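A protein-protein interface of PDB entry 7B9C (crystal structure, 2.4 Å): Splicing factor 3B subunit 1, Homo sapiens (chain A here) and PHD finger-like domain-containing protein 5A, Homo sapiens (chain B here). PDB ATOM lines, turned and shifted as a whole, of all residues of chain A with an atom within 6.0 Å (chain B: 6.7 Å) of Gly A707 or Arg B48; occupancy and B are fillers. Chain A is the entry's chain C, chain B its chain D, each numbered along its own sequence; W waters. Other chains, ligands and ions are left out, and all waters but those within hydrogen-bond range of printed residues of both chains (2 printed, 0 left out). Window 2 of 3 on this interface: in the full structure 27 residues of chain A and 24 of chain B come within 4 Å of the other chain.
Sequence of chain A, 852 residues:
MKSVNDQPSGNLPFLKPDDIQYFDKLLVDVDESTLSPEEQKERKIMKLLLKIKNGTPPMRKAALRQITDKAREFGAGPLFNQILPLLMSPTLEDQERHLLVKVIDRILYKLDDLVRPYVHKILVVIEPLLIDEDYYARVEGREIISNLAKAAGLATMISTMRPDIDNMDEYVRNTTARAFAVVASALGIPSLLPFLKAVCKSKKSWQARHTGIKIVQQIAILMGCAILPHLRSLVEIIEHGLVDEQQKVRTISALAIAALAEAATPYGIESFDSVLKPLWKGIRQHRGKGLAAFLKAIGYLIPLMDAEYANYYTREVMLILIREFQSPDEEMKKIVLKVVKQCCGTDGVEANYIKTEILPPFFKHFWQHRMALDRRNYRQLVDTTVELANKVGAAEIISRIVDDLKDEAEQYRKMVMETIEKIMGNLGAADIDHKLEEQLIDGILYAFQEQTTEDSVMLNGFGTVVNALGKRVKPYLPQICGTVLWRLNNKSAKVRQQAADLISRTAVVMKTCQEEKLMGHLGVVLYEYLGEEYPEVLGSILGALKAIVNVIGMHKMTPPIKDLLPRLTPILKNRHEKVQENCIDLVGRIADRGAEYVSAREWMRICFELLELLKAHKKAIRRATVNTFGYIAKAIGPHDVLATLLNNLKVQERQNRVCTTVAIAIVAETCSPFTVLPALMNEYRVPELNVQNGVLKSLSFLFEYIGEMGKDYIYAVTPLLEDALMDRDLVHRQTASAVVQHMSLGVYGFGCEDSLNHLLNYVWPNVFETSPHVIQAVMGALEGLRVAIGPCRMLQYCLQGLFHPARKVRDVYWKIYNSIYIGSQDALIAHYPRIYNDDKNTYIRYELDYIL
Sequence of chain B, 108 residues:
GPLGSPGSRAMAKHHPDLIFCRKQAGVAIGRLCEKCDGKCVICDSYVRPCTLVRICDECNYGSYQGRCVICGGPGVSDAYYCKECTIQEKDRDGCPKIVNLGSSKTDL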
ATOM      1  N   LEU A 702      10.777 -10.840 -13.910  1.00  0.00           N
ATOM      2  CA  LEU A 702       9.809  -9.908 -13.343  1.00  0.00           C
ATOM      3  C   LEU A 702      10.316  -9.334 -12.029  1.00  0.00           C
ATOM      4  O   LEU A 702      10.259  -8.119 -11.802  1.00  0.00           O
ATOM      5  CB  LEU A 702       8.465 -10.615 -13.142  1.00  0.00           C
ATOM      6  CG  LEU A 702       7.249  -9.795 -12.705  1.00  0.00           C
ATOM      7  CD1 LEU A 702       5.995 -10.332 -13.380  1.00  0.00           C
ATOM      8  CD2 LEU A 702       7.082  -9.809 -11.194  1.00  0.00           C
ATOM      9  N   PHE A 703      10.818 -10.198 -11.146  1.00  0.00           N
ATOM     10  CA  PHE A 703      11.289  -9.709  -9.857  1.00  0.00           C
ATOM     11  C   PHE A 703      12.574  -8.906 -10.008  1.00  0.00           C
ATOM     12  O   PHE A 703      12.721  -7.839  -9.392  1.00  0.00           O
ATOM     13  CB  PHE A 703      11.465 -10.872  -8.884  1.00  0.00           C
ATOM     14  CG  PHE A 703      10.193 -11.259  -8.187  1.00  0.00           C
ATOM     15  CD1 PHE A 703       9.683 -10.474  -7.164  1.00  0.00           C
ATOM     16  CD2 PHE A 703       9.490 -12.390  -8.573  1.00  0.00           C
ATOM     17  CE1 PHE A 703       8.507 -10.820  -6.525  1.00  0.00           C
ATOM     18  CE2 PHE A 703       8.311 -12.742  -7.938  1.00  0.00           C
ATOM     19  CZ  PHE A 703       7.819 -11.957  -6.912  1.00  0.00           C
ATOM     20  N   GLU A 704      13.503  -9.377 -10.851  1.00  0.00           N
ATOM     21  CA  GLU A 704      14.704  -8.589 -11.113  1.00  0.00           C
ATOM     22  C   GLU A 704      14.363  -7.207 -11.664  1.00  0.00           C
ATOM     23  O   GLU A 704      15.056  -6.229 -11.361  1.00  0.00           O
ATOM     24  CB  GLU A 704      15.619  -9.337 -12.082  1.00  0.00           C
ATOM     25  CG  GLU A 704      16.926  -8.619 -12.373  1.00  0.00           C
ATOM     26  CD  GLU A 704      17.795  -9.363 -13.370  1.00  0.00           C
ATOM     27  OE1 GLU A 704      17.262 -10.209 -14.122  1.00  0.00           O
ATOM     28  OE2 GLU A 704      19.016  -9.100 -13.401  1.00  0.00           O
ATOM     29  N   TYR A 705      13.289  -7.100 -12.447  1.00  0.00           N
ATOM     30  CA  TYR A 705      12.949  -5.839 -13.093  1.00  0.00           C
ATOM     31  C   TYR A 705      12.188  -4.904 -12.158  1.00  0.00           C
ATOM     32  O   TYR A 705      12.407  -3.689 -12.187  1.00  0.00           O
ATOM     33  CB  TYR A 705      12.133  -6.112 -14.360  1.00  0.00           C
ATOM     34  CG  TYR A 705      11.719  -4.868 -15.109  1.00  0.00           C
ATOM     35  CD1 TYR A 705      12.638  -4.157 -15.874  1.00  0.00           C
ATOM     36  CD2 TYR A 705      10.410  -4.404 -15.056  1.00  0.00           C
ATOM     37  CE1 TYR A 705      12.265  -3.016 -16.561  1.00  0.00           C
ATOM     38  CE2 TYR A 705      10.026  -3.265 -15.741  1.00  0.00           C
ATOM     39  CZ  TYR A 705      10.959  -2.575 -16.490  1.00  0.00           C
ATOM     40  OH  TYR A 705      10.589  -1.441 -17.177  1.00  0.00           O
ATOM     41  N   ILE A 706      11.293  -5.442 -11.325  1.00  0.00           N
ATOM     42  CA  ILE A 706      10.467  -4.581 -10.482  1.00  0.00           C
ATOM     43  C   ILE A 706      11.126  -4.221  -9.154  1.00  0.00           C
ATOM     44  O   ILE A 706      10.732  -3.220  -8.537  1.00  0.00           O
ATOM     45  CB  ILE A 706       9.084  -5.203 -10.213  1.00  0.00           C
ATOM     46  CG1 ILE A 706       9.199  -6.437  -9.315  1.00  0.00           C
ATOM     47  CG2 ILE A 706       8.377  -5.526 -11.527  1.00  0.00           C
ATOM     48  CD1 ILE A 706       7.863  -7.025  -8.927  1.00  0.00           C
ATOM     49  N   GLY A 707      12.110  -4.998  -8.697  1.00  0.00           N
ATOM     50  CA  GLY A 707      12.867  -4.596  -7.522  1.00  0.00           C
ATOM     51  C   GLY A 707      11.990  -4.431  -6.293  1.00  0.00           C
ATOM     52  O   GLY A 707      11.329  -5.373  -5.839  1.00  0.00           O
ATOM     53  N   GLU A 708      11.979  -3.206  -5.754  1.00  0.00           N
ATOM     54  CA  GLU A 708      11.298  -2.935  -4.490  1.00  0.00           C
ATOM     55  C   GLU A 708       9.805  -3.227  -4.570  1.00  0.00           C
ATOM     56  O   GLU A 708       9.197  -3.641  -3.575  1.00  0.00           O
ATOM     57  CB  GLU A 708      11.541  -1.481  -4.080  1.00  0.00           C
ATOM     58  CG  GLU A 708      10.434  -0.862  -3.243  1.00  0.00           C
ATOM     59  CD  GLU A 708      10.385   0.646  -3.377  1.00  0.00           C
ATOM     60  OE1 GLU A 708      11.126   1.188  -4.228  1.00  0.00           O
ATOM     61  OE2 GLU A 708       9.608   1.289  -2.636  1.00  0.00           O
ATOM     62  N   MET A 709       9.203  -3.032  -5.745  1.00  0.00           N
ATOM     63  CA  MET A 709       7.781  -3.299  -5.931  1.00  0.00           C
ATOM     64  C   MET A 709       7.408  -4.739  -5.592  1.00  0.00           C
ATOM     65  O   MET A 709       6.240  -5.010  -5.289  1.00  0.00           O
ATOM     66  CB  MET A 709       7.397  -2.974  -7.375  1.00  0.00           C
ATOM     67  CG  MET A 709       5.915  -2.982  -7.675  1.00  0.00           C
ATOM     68  SD  MET A 709       5.637  -2.593  -9.411  1.00  0.00           S
ATOM     69  CE  MET A 709       6.226  -0.903  -9.458  1.00  0.00           C
ATOM     70  N   GLY A 710       8.368  -5.664  -5.624  1.00  0.00           N
ATOM     71  CA  GLY A 710       8.108  -7.051  -5.304  1.00  0.00           C
ATOM     72  C   GLY A 710       7.903  -7.363  -3.841  1.00  0.00           C
ATOM     73  O   GLY A 710       7.568  -8.504  -3.509  1.00  0.00           O
ATOM     74  N   LYS A 711       8.081  -6.378  -2.955  1.00  0.00           N
ATOM     75  CA  LYS A 711       7.993  -6.619  -1.517  1.00  0.00           C
ATOM     76  C   LYS A 711       6.619  -7.115  -1.082  1.00  0.00           C
ATOM     77  O   LYS A 711       6.506  -7.734  -0.019  1.00  0.00           O
ATOM     78  CB  LYS A 711       8.343  -5.344  -0.749  1.00  0.00           C
ATOM     79  CG  LYS A 711       7.358  -4.207  -0.954  1.00  0.00           C
ATOM     80  CD  LYS A 711       7.852  -2.926  -0.302  1.00  0.00           C
ATOM     81  CE  LYS A 711       6.981  -1.740  -0.690  1.00  0.00           C
ATOM     82  NZ  LYS A 711       5.551  -1.970  -0.337  1.00  0.00           N
ATOM     83  N   HIS A 742      16.735 -12.882  -7.241  1.00  0.00           N
ATOM     84  CA  HIS A 742      16.247 -11.589  -7.709  1.00  0.00           C
ATOM     85  C   HIS A 742      15.258 -10.978  -6.722  1.00  0.00           C
ATOM     86  O   HIS A 742      15.257  -9.761  -6.517  1.00  0.00           O
ATOM     87  CB  HIS A 742      15.620 -11.734  -9.094  1.00  0.00           C
ATOM     88  CG  HIS A 742      16.602 -12.112 -10.161  1.00  0.00           C
ATOM     89  ND1 HIS A 742      17.781 -11.429 -10.361  1.00  0.00           N
ATOM     90  CD2 HIS A 742      16.580 -13.103 -11.084  1.00  0.00           C
ATOM     91  CE1 HIS A 742      18.444 -11.982 -11.361  1.00  0.00           C
ATOM     92  NE2 HIS A 742      17.737 -13.000 -11.817  1.00  0.00           N
ATOM     93  N   MET A 743      14.426 -11.807  -6.087  1.00  0.00           N
ATOM     94  CA  MET A 743      13.512 -11.317  -5.059  1.00  0.00           C
ATOM     95  C   MET A 743      14.281 -10.712  -3.895  1.00  0.00           C
ATOM     96  O   MET A 743      14.051  -9.561  -3.507  1.00  0.00           O
ATOM     97  CB  MET A 743      12.623 -12.452  -4.551  1.00  0.00           C
ATOM     98  CG  MET A 743      11.503 -12.862  -5.469  1.00  0.00           C
ATOM     99  SD  MET A 743      10.413 -14.027  -4.637  1.00  0.00           S
ATOM    100  CE  MET A 743      11.598 -15.015  -3.747  1.00  0.00           C
ATOM    101  N   GLY A 746      15.935  -7.591  -4.737  1.00  0.00           N
ATOM    102  CA  GLY A 746      15.013  -6.521  -5.069  1.00  0.00           C
ATOM    103  C   GLY A 746      14.270  -5.952  -3.880  1.00  0.00           C
ATOM    104  O   GLY A 746      13.933  -4.765  -3.874  1.00  0.00           O
ATOM    105  N   VAL A 747      14.006  -6.773  -2.862  1.00  0.00           N
ATOM    106  CA  VAL A 747      13.272  -6.331  -1.682  1.00  0.00           C
ATOM    107  C   VAL A 747      14.204  -6.046  -0.509  1.00  0.00           C
ATOM    108  O   VAL A 747      13.739  -5.887   0.626  1.00  0.00           O
ATOM    109  CB  VAL A 747      12.184  -7.348  -1.295  1.00  0.00           C
ATOM    110  CG1 VAL A 747      11.330  -7.684  -2.507  1.00  0.00           C
ATOM    111  CG2 VAL A 747      12.800  -8.611  -0.715  1.00  0.00           C
ATOM    112  N   SER B  45      23.508  -9.239 -17.083  1.00  0.00           N
ATOM    113  CA  SER B  45      22.164  -8.680 -17.028  1.00  0.00           C
ATOM    114  C   SER B  45      22.103  -7.333 -17.737  1.00  0.00           C
ATOM    115  O   SER B  45      23.066  -6.560 -17.743  1.00  0.00           O
ATOM    116  CB  SER B  45      21.698  -8.520 -15.579  1.00  0.00           C
ATOM    117  OG  SER B  45      20.636  -7.588 -15.485  1.00  0.00           O
ATOM    118  N   TYR B  46      20.947  -7.060 -18.337  1.00  0.00           N
ATOM    119  CA  TYR B  46      20.676  -5.793 -18.994  1.00  0.00           C
ATOM    120  C   TYR B  46      19.836  -4.865 -18.128  1.00  0.00           C
ATOM    121  O   TYR B  46      19.447  -3.785 -18.584  1.00  0.00           O
ATOM    122  CB  TYR B  46      19.976  -6.035 -20.333  1.00  0.00           C
ATOM    123  CG  TYR B  46      20.901  -6.458 -21.454  1.00  0.00           C
ATOM    124  CD1 TYR B  46      21.550  -5.512 -22.235  1.00  0.00           C
ATOM    125  CD2 TYR B  46      21.113  -7.802 -21.740  1.00  0.00           C
ATOM    126  CE1 TYR B  46      22.389  -5.888 -23.266  1.00  0.00           C
ATOM    127  CE2 TYR B  46      21.951  -8.189 -22.769  1.00  0.00           C
ATOM    128  CZ  TYR B  46      22.588  -7.226 -23.530  1.00  0.00           C
ATOM    129  OH  TYR B  46      23.424  -7.598 -24.559  1.00  0.00           O
ATOM    130  N   VAL B  47      19.561  -5.257 -16.889  1.00  0.00           N
ATOM    131  CA  VAL B  47      18.666  -4.520 -16.009  1.00  0.00           C
ATOM    132  C   VAL B  47      19.478  -3.561 -15.149  1.00  0.00           C
ATOM    133  O   VAL B  47      20.481  -3.951 -14.538  1.00  0.00           O
ATOM    134  CB  VAL B  47      17.847  -5.483 -15.134  1.00  0.00           C
ATOM    135  CG1 VAL B  47      16.899  -4.713 -14.230  1.00  0.00           C
ATOM    136  CG2 VAL B  47      17.085  -6.466 -16.006  1.00  0.00           C
ATOM    137  N   ARG B  48      19.047  -2.300 -15.120  1.00  0.00           N
ATOM    138  CA  ARG B  48      19.485  -1.250 -14.207  1.00  0.00           C
ATOM    139  C   ARG B  48      21.001  -1.147 -14.062  1.00  0.00           C
ATOM    140  O   ARG B  48      21.559  -1.602 -13.054  1.00  0.00           O
ATOM    141  CB  ARG B  48      18.847  -1.465 -12.833  1.00  0.00           C
ATOM    142  CG  ARG B  48      17.625  -0.599 -12.583  1.00  0.00           C
ATOM    143  CD  ARG B  48      17.192  -0.655 -11.126  1.00  0.00           C
ATOM    144  NE  ARG B  48      16.834  -2.011 -10.723  1.00  0.00           N
ATOM    145  CZ  ARG B  48      15.667  -2.586 -10.997  1.00  0.00           C
ATOM    146  NH1 ARG B  48      15.425  -3.825 -10.593  1.00  0.00           N
ATOM    147  NH2 ARG B  48      14.744  -1.920 -11.677  1.00  0.00           N
ATOM    148  N   PRO B  49      21.699  -0.560 -15.033  1.00  0.00           N
ATOM    149  CA  PRO B  49      23.101  -0.193 -14.805  1.00  0.00           C
ATOM    150  C   PRO B  49      23.210   0.775 -13.637  1.00  0.00           C
ATOM    151  O   PRO B  49      22.308   1.575 -13.378  1.00  0.00           O
ATOM    152  CB  PRO B  49      23.519   0.464 -16.126  1.00  0.00           C
ATOM    153  CG  PRO B  49      22.580  -0.116 -17.146  1.00  0.00           C
ATOM    154  CD  PRO B  49      21.274  -0.295 -16.419  1.00  0.00           C
ATOM    155  N   CYS B  50      24.332   0.702 -12.924  1.00  0.00           N
ATOM    156  CA  CYS B  50      24.460   1.438 -11.675  1.00  0.00           C
ATOM    157  C   CYS B  50      25.808   2.149 -11.561  1.00  0.00           C
ATOM    158  O   CYS B  50      25.859   3.382 -11.580  1.00  0.00           O
ATOM    159  CB  CYS B  50      24.251   0.481 -10.497  1.00  0.00           C
ATOM    160  SG  CYS B  50      24.556   1.194  -8.875  1.00  0.00           S
ATOM    161  N   THR B  51      26.902   1.395 -11.458  1.00  0.00           N
ATOM    162  CA  THR B  51      28.217   1.962 -11.183  1.00  0.00           C
ATOM    163  C   THR B  51      29.168   1.750 -12.356  1.00  0.00           C
ATOM    164  O   THR B  51      29.225   0.663 -12.940  1.00  0.00           O
ATOM    165  CB  THR B  51      28.813   1.359  -9.906  1.00  0.00           C
ATOM    166  OG1 THR B  51      27.938   1.624  -8.803  1.00  0.00           O
ATOM    167  CG2 THR B  51      30.179   1.960  -9.606  1.00  0.00           C
ATOM    168  N   TYR B  80      29.097  -0.726 -17.292  1.00  0.00           N
ATOM    169  CA  TYR B  80      28.497  -0.522 -15.982  1.00  0.00           C
ATOM    170  C   TYR B  80      28.320  -1.857 -15.275  1.00  0.00           C
ATOM    171  O   TYR B  80      28.116  -2.895 -15.910  1.00  0.00           O
ATOM    172  CB  TYR B  80      27.129   0.175 -16.087  1.00  0.00           C
ATOM    173  CG  TYR B  80      27.193   1.681 -16.195  1.00  0.00           C
ATOM    174  CD1 TYR B  80      27.411   2.302 -17.420  1.00  0.00           C
ATOM    175  CD2 TYR B  80      27.023   2.484 -15.072  1.00  0.00           C
ATOM    176  CE1 TYR B  80      27.467   3.680 -17.522  1.00  0.00           C
ATOM    177  CE2 TYR B  80      27.078   3.863 -15.163  1.00  0.00           C
ATOM    178  CZ  TYR B  80      27.297   4.456 -16.390  1.00  0.00           C
ATOM    179  OH  TYR B  80      27.352   5.828 -16.478  1.00  0.00           O
ATOM    180  N   TYR B  81      28.407  -1.818 -13.950  1.00  0.00           N
ATOM    181  CA  TYR B  81      27.948  -2.919 -13.118  1.00  0.00           C
ATOM    182  C   TYR B  81      26.453  -2.761 -12.878  1.00  0.00           C
ATOM    183  O   TYR B  81      25.961  -1.645 -12.705  1.00  0.00           O
ATOM    184  CB  TYR B  81      28.685  -2.940 -11.779  1.00  0.00           C
ATOM    185  CG  TYR B  81      30.160  -3.254 -11.860  1.00  0.00           C
ATOM    186  CD1 TYR B  81      30.607  -4.559 -12.021  1.00  0.00           C
ATOM    187  CD2 TYR B  81      31.107  -2.246 -11.754  1.00  0.00           C
ATOM    188  CE1 TYR B  81      31.957  -4.848 -12.079  1.00  0.00           C
ATOM    189  CE2 TYR B  81      32.457  -2.525 -11.811  1.00  0.00           C
ATOM    190  CZ  TYR B  81      32.877  -3.827 -11.974  1.00  0.00           C
ATOM    191  OH  TYR B  81      34.222  -4.104 -12.031  1.00  0.00           O
ATOM    192  N   CYS B  82      25.730  -3.878 -12.865  1.00  0.00           N
ATOM    193  CA  CYS B  82      24.297  -3.800 -12.625  1.00  0.00           C
ATOM    194  C   CYS B  82      24.021  -3.471 -11.156  1.00  0.00           C
ATOM    195  O   CYS B  82      24.919  -3.458 -10.308  1.00  0.00           O
ATOM    196  CB  CYS B  82      23.611  -5.105 -13.036  1.00  0.00           C
ATOM    197  SG  CYS B  82      23.830  -6.471 -11.895  1.00  0.00           S
ATOM    198  N   LYS B  83      22.752  -3.185 -10.862  1.00  0.00           N
ATOM    199  CA  LYS B  83      22.369  -2.833  -9.498  1.00  0.00           C
ATOM    200  C   LYS B  83      22.586  -4.004  -8.548  1.00  0.00           C
ATOM    201  O   LYS B  83      23.022  -3.815  -7.407  1.00  0.00           O
ATOM    202  CB  LYS B  83      20.910  -2.371  -9.465  1.00  0.00           C
ATOM    203  CG  LYS B  83      20.449  -1.823  -8.120  1.00  0.00           C
ATOM    204  CD  LYS B  83      21.158  -0.521  -7.782  1.00  0.00           C
ATOM    205  CE  LYS B  83      20.875  -0.082  -6.352  1.00  0.00           C
ATOM    206  NZ  LYS B  83      21.634   1.150  -5.980  1.00  0.00           N
ATOM    207  N   GLU B  84      22.298  -5.225  -9.006  1.00  0.00           N
ATOM    208  CA  GLU B  84      22.502  -6.396  -8.161  1.00  0.00           C
ATOM    209  C   GLU B  84      23.974  -6.601  -7.836  1.00  0.00           C
ATOM    210  O   GLU B  84      24.311  -7.043  -6.732  1.00  0.00           O
ATOM    211  CB  GLU B  84      21.932  -7.644  -8.838  1.00  0.00           C
ATOM    212  CG  GLU B  84      20.416  -7.640  -8.988  1.00  0.00           C
ATOM    213  CD  GLU B  84      19.841  -9.024  -9.257  1.00  0.00           C
ATOM    214  OE1 GLU B  84      20.613  -9.943  -9.609  1.00  0.00           O
ATOM    215  OE2 GLU B  84      18.612  -9.192  -9.112  1.00  0.00           O
HETATM  216  O   HOH W   1      15.776  -5.843  -8.613  1.00  0.00           O
HETATM  217  O   HOH W   2      20.613  -7.384 -12.335  1.00  0.00           O
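Of the 12 printed residues of chain B, 4 touch a printed residue of chain A.
Printed residues of chain B that touch a printed residue of chain A: Ser B45, Val B47, Arg B48 and Glu B84.
Hydrophobic or aromatic side chains of chain B that line the printed part of chain A: Val B47.
Hydrophobic or aromatic side chains of chain A within 4 Å of the printed part of chain B: His A742.
Of the printed residues of chain B, Gly A707 touches Arg B48 (3.99 Å).
Printed residues of chain A within 4 Å of Arg B48: Glu A704, Tyr A705 and Gly A707.
Of the printed residues of chain B, Tyr A705 touches Arg B48.
Printed residues of chain B within 4 Å of His A742: Glu B84 (2.7 Å).
Lys A711 touches none of the printed residues of chain B.
Cys B50 touches none of the printed residues of chain A.
The nearest printed residue of chain B that does not touch Gly A707 is Val B47 (7.3 Å).
The nearest printed residue of chain A that does not touch Arg B48 is Ile A706 (4.5 Å).
The nearest printed residue of chain B that does not touch His A742 is Ser B45 (6.4 Å).
CG1 of Val B47 touches O of Glu A704 (3.7 Å).
Glu B84 touches Glu A704.
Gly A707 touches Arg B48 (N to NH1, 3.99 Å).
Water W2 lies within hydrogen-bond range of OE2 of Glu A704 (2.6 Å) and OG of Ser B45 (3.2 Å).
Water W1 lies within hydrogen-bond range of the guanidinium group (NH1) of Arg B48 (2.8 Å) and the backbone carbonyl oxygen (O) of Glu A704 (2.9 Å).
The backbone carbonyl oxygen (O) of Glu A704 is in hydrogen-bond range of the guanidinium group (NH1) of Arg B48 (2.6 Å).
ND1 of His A742 is in hydrogen-bond range of OE2 of Glu B84 (2.7 Å).
NH2 of Arg B48 is in hydrogen-bond range of O of Tyr A705 (3.0 Å).
OE2 of Glu A704 lies within hydrogen-bond range of OG of Ser B45, at 3.0 Å.
The side-chain hydroxyl (OG) of Ser B45 lies within hydrogen-bond range of the backbone NH (N) of Val B47 (2.9 Å).
N of Glu B84 sits close to SG of Cys B82 (3.5 Å).
The backbone carbonyl oxygen (O) of Arg B48 is in hydrogen-bond range of the backbone NH (N) of Lys B83, at 3.0 Å.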
